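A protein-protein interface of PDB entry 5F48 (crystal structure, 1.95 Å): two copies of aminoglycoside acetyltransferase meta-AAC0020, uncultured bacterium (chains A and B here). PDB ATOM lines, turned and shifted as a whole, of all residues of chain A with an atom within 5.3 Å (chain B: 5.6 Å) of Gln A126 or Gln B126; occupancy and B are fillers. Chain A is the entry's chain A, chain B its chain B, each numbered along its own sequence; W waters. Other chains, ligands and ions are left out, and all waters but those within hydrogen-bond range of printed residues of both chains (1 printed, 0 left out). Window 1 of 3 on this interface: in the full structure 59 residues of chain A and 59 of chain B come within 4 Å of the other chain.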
ATOM      1  N   TYR A  88       2.240 -35.870  20.080  1.00  0.00           N
ATOM      2  CA  TYR A  88       2.728 -35.386  18.799  1.00  0.00           C
ATOM      3  C   TYR A  88       3.943 -36.220  18.430  1.00  0.00           C
ATOM      4  O   TYR A  88       5.005 -36.068  19.032  1.00  0.00           O
ATOM      5  CB  TYR A  88       3.098 -33.901  18.912  1.00  0.00           C
ATOM      6  CG  TYR A  88       3.713 -33.251  17.682  1.00  0.00           C
ATOM      7  CD1 TYR A  88       3.585 -33.805  16.413  1.00  0.00           C
ATOM      8  CD2 TYR A  88       4.425 -32.077  17.803  1.00  0.00           C
ATOM      9  CE1 TYR A  88       4.148 -33.192  15.307  1.00  0.00           C
ATOM     10  CE2 TYR A  88       4.980 -31.463  16.714  1.00  0.00           C
ATOM     11  CZ  TYR A  88       4.843 -32.022  15.470  1.00  0.00           C
ATOM     12  OH  TYR A  88       5.419 -31.380  14.407  1.00  0.00           O
ATOM     13  N   ILE A  89       3.782 -37.118  17.468  1.00  0.00           N
ATOM     14  CA  ILE A  89       4.914 -37.858  16.939  1.00  0.00           C
ATOM     15  C   ILE A  89       5.713 -36.931  16.041  1.00  0.00           C
ATOM     16  O   ILE A  89       5.194 -36.426  15.043  1.00  0.00           O
ATOM     17  CB  ILE A  89       4.456 -39.117  16.165  1.00  0.00           C
ATOM     18  CG1 ILE A  89       3.718 -40.063  17.115  1.00  0.00           C
ATOM     19  CG2 ILE A  89       5.649 -39.797  15.478  1.00  0.00           C
ATOM     20  CD1 ILE A  89       3.173 -41.359  16.465  1.00  0.00           C
ATOM     21  N   PHE A 124      -1.071 -37.543  16.876  1.00  0.00           N
ATOM     22  CA  PHE A 124      -1.001 -37.060  15.508  1.00  0.00           C
ATOM     23  C   PHE A 124       0.437 -37.010  15.044  1.00  0.00           C
ATOM     24  O   PHE A 124       1.361 -36.999  15.855  1.00  0.00           O
ATOM     25  CB  PHE A 124      -1.685 -35.686  15.363  1.00  0.00           C
ATOM     26  CG  PHE A 124      -1.035 -34.567  16.151  1.00  0.00           C
ATOM     27  CD1 PHE A 124      -1.410 -34.310  17.463  1.00  0.00           C
ATOM     28  CD2 PHE A 124      -0.097 -33.735  15.556  1.00  0.00           C
ATOM     29  CE1 PHE A 124      -0.824 -33.252  18.181  1.00  0.00           C
ATOM     30  CE2 PHE A 124       0.484 -32.677  16.266  1.00  0.00           C
ATOM     31  CZ  PHE A 124       0.118 -32.438  17.576  1.00  0.00           C
ATOM     32  N   VAL A 125       0.605 -36.991  13.730  1.00  0.00           N
ATOM     33  CA  VAL A 125       1.900 -37.087  13.084  1.00  0.00           C
ATOM     34  C   VAL A 125       1.761 -36.461  11.701  1.00  0.00           C
ATOM     35  O   VAL A 125       0.656 -36.403  11.154  1.00  0.00           O
ATOM     36  CB  VAL A 125       2.389 -38.559  12.982  1.00  0.00           C
ATOM     37  CG1 VAL A 125       1.519 -39.356  12.033  1.00  0.00           C
ATOM     38  CG2 VAL A 125       3.838 -38.611  12.536  1.00  0.00           C
ATOM     39  N   GLN A 126       2.865 -35.973  11.141  1.00  0.00           N
ATOM     40  CA  GLN A 126       2.801 -35.250   9.882  1.00  0.00           C
ATOM     41  C   GLN A 126       3.884 -35.660   8.909  1.00  0.00           C
ATOM     42  O   GLN A 126       4.939 -36.153   9.305  1.00  0.00           O
ATOM     43  CB  GLN A 126       2.889 -33.753  10.153  1.00  0.00           C
ATOM     44  CG  GLN A 126       1.832 -33.284  11.142  1.00  0.00           C
ATOM     45  CD  GLN A 126       1.810 -31.784  11.302  1.00  0.00           C
ATOM     46  OE1 GLN A 126       2.830 -31.124  11.139  1.00  0.00           O
ATOM     47  NE2 GLN A 126       0.637 -31.234  11.592  1.00  0.00           N
ATOM     48  N   ALA A 127       3.623 -35.450   7.630  1.00  0.00           N
ATOM     49  CA  ALA A 127       4.604 -35.725   6.593  1.00  0.00           C
ATOM     50  C   ALA A 127       4.568 -34.619   5.548  1.00  0.00           C
ATOM     51  O   ALA A 127       3.527 -34.031   5.327  1.00  0.00           O
ATOM     52  CB  ALA A 127       4.333 -37.089   5.944  1.00  0.00           C
ATOM     53  N   ASP A 128       5.693 -34.337   4.897  1.00  0.00           N
ATOM     54  CA  ASP A 128       5.691 -33.355   3.824  1.00  0.00           C
ATOM     55  C   ASP A 128       4.897 -33.900   2.641  1.00  0.00           C
ATOM     56  O   ASP A 128       4.954 -35.097   2.345  1.00  0.00           O
ATOM     57  CB  ASP A 128       7.119 -33.003   3.399  1.00  0.00           C
ATOM     58  CG  ASP A 128       7.905 -32.299   4.498  1.00  0.00           C
ATOM     59  OD1 ASP A 128       7.285 -31.736   5.425  1.00  0.00           O
ATOM     60  OD2 ASP A 128       9.149 -32.314   4.432  1.00  0.00           O
ATOM     61  N   TYR A 138       2.189 -43.754   6.295  1.00  0.00           N
ATOM     62  CA  TYR A 138       1.189 -43.353   7.293  1.00  0.00           C
ATOM     63  C   TYR A 138      -0.211 -43.784   6.868  1.00  0.00           C
ATOM     64  O   TYR A 138      -1.030 -44.184   7.695  1.00  0.00           O
ATOM     65  CB  TYR A 138       1.241 -41.842   7.546  1.00  0.00           C
ATOM     66  CG  TYR A 138       2.449 -41.470   8.361  1.00  0.00           C
ATOM     67  CD1 TYR A 138       2.663 -42.048   9.604  1.00  0.00           C
ATOM     68  CD2 TYR A 138       3.401 -40.573   7.873  1.00  0.00           C
ATOM     69  CE1 TYR A 138       3.785 -41.731  10.358  1.00  0.00           C
ATOM     70  CE2 TYR A 138       4.527 -40.240   8.627  1.00  0.00           C
ATOM     71  CZ  TYR A 138       4.711 -40.824   9.865  1.00  0.00           C
ATOM     72  OH  TYR A 138       5.837 -40.514  10.614  1.00  0.00           O
ATOM     73  N   VAL A 149      -2.642 -29.543   5.378  1.00  0.00           N
ATOM     74  CA  VAL A 149      -2.378 -28.338   6.159  1.00  0.00           C
ATOM     75  C   VAL A 149      -1.199 -27.569   5.598  1.00  0.00           C
ATOM     76  O   VAL A 149      -0.410 -28.098   4.809  1.00  0.00           O
ATOM     77  CB  VAL A 149      -2.119 -28.664   7.641  1.00  0.00           C
ATOM     78  CG1 VAL A 149      -3.337 -29.361   8.248  1.00  0.00           C
ATOM     79  CG2 VAL A 149      -0.902 -29.515   7.783  1.00  0.00           C
ATOM     80  N   VAL A 150      -1.102 -26.303   5.975  1.00  0.00           N
ATOM     81  CA  VAL A 150       0.024 -25.489   5.563  1.00  0.00           C
ATOM     82  C   VAL A 150       0.821 -25.146   6.816  1.00  0.00           C
ATOM     83  O   VAL A 150       0.267 -24.744   7.826  1.00  0.00           O
ATOM     84  CB  VAL A 150      -0.410 -24.212   4.827  1.00  0.00           C
ATOM     85  CG1 VAL A 150       0.799 -23.426   4.385  1.00  0.00           C
ATOM     86  CG2 VAL A 150      -1.259 -24.567   3.624  1.00  0.00           C
ATOM     87  N   HIS A 151       2.121 -25.356   6.732  1.00  0.00           N
ATOM     88  CA  HIS A 151       3.045 -25.189   7.838  1.00  0.00           C
ATOM     89  C   HIS A 151       3.828 -23.902   7.620  1.00  0.00           C
ATOM     90  O   HIS A 151       4.509 -23.767   6.612  1.00  0.00           O
ATOM     91  CB  HIS A 151       3.974 -26.417   7.889  1.00  0.00           C
ATOM     92  CG  HIS A 151       5.028 -26.369   8.952  1.00  0.00           C
ATOM     93  ND1 HIS A 151       4.794 -26.765  10.250  1.00  0.00           N
ATOM     94  CD2 HIS A 151       6.344 -26.043   8.889  1.00  0.00           C
ATOM     95  CE1 HIS A 151       5.913 -26.655  10.949  1.00  0.00           C
ATOM     96  NE2 HIS A 151       6.867 -26.217  10.146  1.00  0.00           N
ATOM     97  N   PHE A 152       3.708 -22.947   8.537  1.00  0.00           N
ATOM     98  CA  PHE A 152       4.484 -21.715   8.430  1.00  0.00           C
ATOM     99  C   PHE A 152       5.538 -21.676   9.517  1.00  0.00           C
ATOM    100  O   PHE A 152       5.247 -22.013  10.667  1.00  0.00           O
ATOM    101  CB  PHE A 152       3.608 -20.487   8.581  1.00  0.00           C
ATOM    102  CG  PHE A 152       2.518 -20.377   7.556  1.00  0.00           C
ATOM    103  CD1 PHE A 152       2.732 -19.689   6.373  1.00  0.00           C
ATOM    104  CD2 PHE A 152       1.280 -20.936   7.793  1.00  0.00           C
ATOM    105  CE1 PHE A 152       1.730 -19.563   5.434  1.00  0.00           C
ATOM    106  CE2 PHE A 152       0.273 -20.827   6.848  1.00  0.00           C
ATOM    107  CZ  PHE A 152       0.505 -20.128   5.676  1.00  0.00           C
ATOM    108  N   TYR B  88       5.767 -23.954  19.173  1.00  0.00           N
ATOM    109  CA  TYR B  88       4.645 -24.397  18.357  1.00  0.00           C
ATOM    110  C   TYR B  88       3.425 -23.591  18.776  1.00  0.00           C
ATOM    111  O   TYR B  88       2.902 -23.815  19.852  1.00  0.00           O
ATOM    112  CB  TYR B  88       4.410 -25.898  18.579  1.00  0.00           C
ATOM    113  CG  TYR B  88       3.233 -26.535  17.860  1.00  0.00           C
ATOM    114  CD1 TYR B  88       2.655 -25.963  16.717  1.00  0.00           C
ATOM    115  CD2 TYR B  88       2.715 -27.725  18.321  1.00  0.00           C
ATOM    116  CE1 TYR B  88       1.582 -26.582  16.075  1.00  0.00           C
ATOM    117  CE2 TYR B  88       1.667 -28.336  17.699  1.00  0.00           C
ATOM    118  CZ  TYR B  88       1.093 -27.774  16.587  1.00  0.00           C
ATOM    119  OH  TYR B  88       0.039 -28.465  16.012  1.00  0.00           O
ATOM    120  N   ILE B  89       3.007 -22.639  17.951  1.00  0.00           N
ATOM    121  CA  ILE B  89       1.752 -21.922  18.162  1.00  0.00           C
ATOM    122  C   ILE B  89       0.606 -22.843  17.824  1.00  0.00           C
ATOM    123  O   ILE B  89       0.497 -23.311  16.690  1.00  0.00           O
ATOM    124  CB  ILE B  89       1.665 -20.663  17.278  1.00  0.00           C
ATOM    125  CG1 ILE B  89       2.803 -19.695  17.610  1.00  0.00           C
ATOM    126  CG2 ILE B  89       0.265 -20.006  17.392  1.00  0.00           C
ATOM    127  CD1 ILE B  89       2.905 -18.490  16.645  1.00  0.00           C
ATOM    128  N   PHE B 124       6.803 -22.127  14.814  1.00  0.00           N
ATOM    129  CA  PHE B 124       5.952 -22.517  13.697  1.00  0.00           C
ATOM    130  C   PHE B 124       4.477 -22.593  14.095  1.00  0.00           C
ATOM    131  O   PHE B 124       4.114 -22.673  15.267  1.00  0.00           O
ATOM    132  CB  PHE B 124       6.419 -23.841  13.049  1.00  0.00           C
ATOM    133  CG  PHE B 124       6.328 -25.058  13.944  1.00  0.00           C
ATOM    134  CD1 PHE B 124       7.399 -25.429  14.744  1.00  0.00           C
ATOM    135  CD2 PHE B 124       5.191 -25.850  13.948  1.00  0.00           C
ATOM    136  CE1 PHE B 124       7.317 -26.544  15.558  1.00  0.00           C
ATOM    137  CE2 PHE B 124       5.113 -26.977  14.752  1.00  0.00           C
ATOM    138  CZ  PHE B 124       6.173 -27.324  15.556  1.00  0.00           C
ATOM    139  N   VAL B 125       3.636 -22.525  13.078  1.00  0.00           N
ATOM    140  CA  VAL B 125       2.195 -22.470  13.244  1.00  0.00           C
ATOM    141  C   VAL B 125       1.606 -23.081  11.995  1.00  0.00           C
ATOM    142  O   VAL B 125       2.246 -23.086  10.933  1.00  0.00           O
ATOM    143  CB  VAL B 125       1.686 -21.027  13.438  1.00  0.00           C
ATOM    144  CG1 VAL B 125       1.927 -20.199  12.169  1.00  0.00           C
ATOM    145  CG2 VAL B 125       0.204 -21.009  13.816  1.00  0.00           C
ATOM    146  N   GLN B 126       0.412 -23.640  12.120  1.00  0.00           N
ATOM    147  CA  GLN B 126      -0.195 -24.316  10.991  1.00  0.00           C
ATOM    148  C   GLN B 126      -1.620 -23.840  10.757  1.00  0.00           C
ATOM    149  O   GLN B 126      -2.267 -23.278  11.647  1.00  0.00           O
ATOM    150  CB  GLN B 126      -0.171 -25.827  11.201  1.00  0.00           C
ATOM    151  CG  GLN B 126       1.195 -26.342  11.679  1.00  0.00           C
ATOM    152  CD  GLN B 126       1.338 -27.857  11.555  1.00  0.00           C
ATOM    153  OE1 GLN B 126       0.408 -28.608  11.847  1.00  0.00           O
ATOM    154  NE2 GLN B 126       2.501 -28.307  11.097  1.00  0.00           N
ATOM    155  N   ALA B 127      -2.095 -24.059   9.543  1.00  0.00           N
ATOM    156  CA  ALA B 127      -3.479 -23.772   9.211  1.00  0.00           C
ATOM    157  C   ALA B 127      -3.976 -24.794   8.197  1.00  0.00           C
ATOM    158  O   ALA B 127      -3.187 -25.332   7.405  1.00  0.00           O
ATOM    159  CB  ALA B 127      -3.615 -22.354   8.677  1.00  0.00           C
ATOM    160  N   ASP B 128      -5.269 -25.100   8.240  1.00  0.00           N
ATOM    161  CA  ASP B 128      -5.850 -26.021   7.270  1.00  0.00           C
ATOM    162  C   ASP B 128      -5.790 -25.441   5.858  1.00  0.00           C
ATOM    163  O   ASP B 128      -6.030 -24.260   5.651  1.00  0.00           O
ATOM    164  CB  ASP B 128      -7.296 -26.357   7.644  1.00  0.00           C
ATOM    165  CG  ASP B 128      -7.400 -27.085   8.980  1.00  0.00           C
ATOM    166  OD1 ASP B 128      -6.339 -27.385   9.582  1.00  0.00           O
ATOM    167  OD2 ASP B 128      -8.538 -27.370   9.421  1.00  0.00           O
ATOM    168  N   TYR B 138      -1.629 -15.676   7.857  1.00  0.00           N
ATOM    169  CA  TYR B 138      -0.263 -16.075   8.175  1.00  0.00           C
ATOM    170  C   TYR B 138       0.706 -15.559   7.126  1.00  0.00           C
ATOM    171  O   TYR B 138       1.796 -15.109   7.454  1.00  0.00           O
ATOM    172  CB  TYR B 138      -0.165 -17.598   8.319  1.00  0.00           C
ATOM    173  CG  TYR B 138      -0.765 -18.041   9.623  1.00  0.00           C
ATOM    174  CD1 TYR B 138      -0.282 -17.536  10.825  1.00  0.00           C
ATOM    175  CD2 TYR B 138      -1.829 -18.936   9.660  1.00  0.00           C
ATOM    176  CE1 TYR B 138      -0.833 -17.911  12.029  1.00  0.00           C
ATOM    177  CE2 TYR B 138      -2.388 -19.319  10.867  1.00  0.00           C
ATOM    178  CZ  TYR B 138      -1.884 -18.808  12.045  1.00  0.00           C
ATOM    179  OH  TYR B 138      -2.434 -19.172  13.244  1.00  0.00           O
ATOM    180  N   VAL B 149       1.965 -29.787   4.006  1.00  0.00           N
ATOM    181  CA  VAL B 149       2.115 -30.928   4.897  1.00  0.00           C
ATOM    182  C   VAL B 149       0.798 -31.697   4.917  1.00  0.00           C
ATOM    183  O   VAL B 149      -0.270 -31.103   4.721  1.00  0.00           O
ATOM    184  CB  VAL B 149       2.502 -30.449   6.326  1.00  0.00           C
ATOM    185  CG1 VAL B 149       2.261 -31.522   7.370  1.00  0.00           C
ATOM    186  CG2 VAL B 149       3.948 -29.967   6.349  1.00  0.00           C
ATOM    187  N   VAL B 150       0.871 -33.012   5.100  1.00  0.00           N
ATOM    188  CA  VAL B 150      -0.309 -33.806   5.371  1.00  0.00           C
ATOM    189  C   VAL B 150      -0.311 -34.195   6.846  1.00  0.00           C
ATOM    190  O   VAL B 150       0.706 -34.681   7.386  1.00  0.00           O
ATOM    191  CB  VAL B 150      -0.370 -35.070   4.483  1.00  0.00           C
ATOM    192  CG1 VAL B 150      -1.645 -35.842   4.734  1.00  0.00           C
ATOM    193  CG2 VAL B 150      -0.262 -34.676   3.032  1.00  0.00           C
ATOM    194  N   HIS B 151      -1.451 -33.986   7.490  1.00  0.00           N
ATOM    195  CA  HIS B 151      -1.593 -34.203   8.918  1.00  0.00           C
ATOM    196  C   HIS B 151      -2.450 -35.430   9.181  1.00  0.00           C
ATOM    197  O   HIS B 151      -3.622 -35.465   8.774  1.00  0.00           O
ATOM    198  CB  HIS B 151      -2.212 -32.949   9.551  1.00  0.00           C
ATOM    199  CG  HIS B 151      -2.630 -33.103  10.980  1.00  0.00           C
ATOM    200  ND1 HIS B 151      -1.775 -32.868  12.037  1.00  0.00           N
ATOM    201  CD2 HIS B 151      -3.834 -33.401  11.529  1.00  0.00           C
ATOM    202  CE1 HIS B 151      -2.427 -33.041  13.174  1.00  0.00           C
ATOM    203  NE2 HIS B 151      -3.677 -33.367  12.896  1.00  0.00           N
ATOM    204  N   PHE B 152      -1.881 -36.423   9.865  1.00  0.00           N
ATOM    205  CA  PHE B 152      -2.612 -37.643  10.201  1.00  0.00           C
ATOM    206  C   PHE B 152      -2.921 -37.711  11.684  1.00  0.00           C
ATOM    207  O   PHE B 152      -2.073 -37.356  12.504  1.00  0.00           O
ATOM    208  CB  PHE B 152      -1.807 -38.898   9.814  1.00  0.00           C
ATOM    209  CG  PHE B 152      -1.453 -38.976   8.372  1.00  0.00           C
ATOM    210  CD1 PHE B 152      -2.310 -39.567   7.473  1.00  0.00           C
ATOM    211  CD2 PHE B 152      -0.232 -38.505   7.916  1.00  0.00           C
ATOM    212  CE1 PHE B 152      -1.980 -39.662   6.136  1.00  0.00           C
ATOM    213  CE2 PHE B 152       0.101 -38.598   6.569  1.00  0.00           C
ATOM    214  CZ  PHE B 152      -0.772 -39.184   5.688  1.00  0.00           C
HETATM  215  O   HOH W   1      -0.853 -29.571   2.021  1.00  0.00           O
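Water W1 lies within hydrogen-bond range of O of Val B149 (3.2 Å) and O of Val A149 (3.2 Å).
Gln A126 touches just these residues of chain B: Gln B126, Val B149, Val B150 and His B151. Gln B126 touches just these residues of chain A: Gln A126, Val A150 and His A151. Of the printed residues of chain A, His B151 touches Phe A124, Val A125, Gln A126 and Val A149. Printed residues of chain B within 4 Å of Asp A128: Val B149 (3.9 Å). Printed residues of chain B within 4 Å of Phe A152: Phe B124 (3.2 Å), Val B125 (2.8 Å) and Tyr B138 (3.6 Å). Printed residues of chain A within 4 Å of Val B149: Gln A126 (3.6 Å), Ala A127 (3.4 Å), Asp A128 (3.9 Å), Val A149 (2.9 Å) and His A151 (3.9 Å). Printed residues of chain B within 4 Å of Val A125: His B151 and Phe B152. The nearest residue of chain B that does not touch Gln A126 is Phe B152 (4.8 Å). The nearest residue of chain A that does not touch Gln B126 is Val A149 (4.4 Å). The nearest printed residue of chain B that does not touch Val A149 is Gln B126 (4.4 Å).
Among the printed residues, pairs that only touch across the chains: Phe A124 with His B151 (3.4 Å), Phe A124 with Phe B152 (3.2 Å), Val A125 with His B151 (3.8 Å), Gln A126 with Val B149 (3.6 Å), Gln A126 with Val B150 (3.3 Å), Ala A127 with Val B149 (3.4 Å), Asp A128 with Val B149 (3.9 Å), Tyr A138 with Phe B152 (3.6 Å), Val A149 with Ala B127 (3.4 Å), Val A149 with Asp B128 (3.8 Å), Val A149 with His B151 (3.98 Å), Val A150 with Gln B126 (3.2 Å), His A151 with Phe B124 (3.2 Å), His A151 with Val B125 (3.8 Å), His A151 with Val B149 (3.9 Å), Phe A152 with Phe B124 (3.2 Å) and Phe A152 with Tyr B138 (3.6 Å).
Of the 12 printed residues of chain B, 10 touch a printed residue of chain A. Hydrophobic or aromatic side chains of chain B that line the printed part of chain A: Phe B124, Val B125, Tyr B138, Val B149, His B151 and Phe B152. Along chain B the printed residues that touch a printed residue of chain A span positions 124 to 152. Printed residues of chain A that touch a printed residue of chain B: Phe A124, Val A125, Gln A126, Ala A127, Asp A128, Tyr A138, Val A149, Val A150, His A151 and Phe A152. Hydrophobic or aromatic side chains of chain A within 4 Å of the printed part of chain B: Phe A124, Tyr A138, Val A149, Val A150, His A151 and Phe A152.
Ala A127 touches Val B149, and with the chains exchanged Val A149 touches Ala B127. Ala A127 touches Val B150, and with the chains exchanged Val A150 touches Ala B127. Tyr A138 touches Phe B152, and with the chains exchanged Phe A152 touches Tyr B138. Val B149 touches its own counterpart, Val A149. Positions printed for both chains: 88, 89, 124, 125, 126, 127, 128, 138, 149, 150, 151 and 152. Of the 25 pairs that touch across the chains among the printed residues, 24 have their exchanged pair printed and touching as well.
The backbone NH (N) of Phe B152 sits at hydrogen-bond distance from the backbone carbonyl oxygen (O) of Val A125, at 2.8 Å. The side-chain amide nitrogen of Gln A126 sits at hydrogen-bond distance from the side-chain amide oxygen of Gln B126 (2.6 Å). ND1 of His B151 is in hydrogen-bond range of NE2 of Gln A126, 2.9 Å away. The backbone carbonyl oxygen (O) of Ala A127 is in hydrogen-bond range of the backbone NH (N) of Val B150, at 2.9 Å. The backbone carbonyl oxygen (O) of Val B149 is in hydrogen-bond range of the backbone NH (N) of Val A149 (2.9 Å). N of Val A150 sits at hydrogen-bond distance from O of Ala B127. The side-chain amide nitrogen of Gln B126 lies within hydrogen-bond range of a ring nitrogen (ND1) of His A151 (2.9 Å). The backbone carbonyl oxygen (O) of Val B125 is in hydrogen-bond range of the backbone NH (N) of Phe A152 (2.8 Å).
The backbone NH of Ile A89 sits at hydrogen-bond distance from the backbone carbonyl oxygen of Phe A124 (2.9 Å). N of Ile B89 lies within hydrogen-bond range of O of Phe B124, 2.9 Å away.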
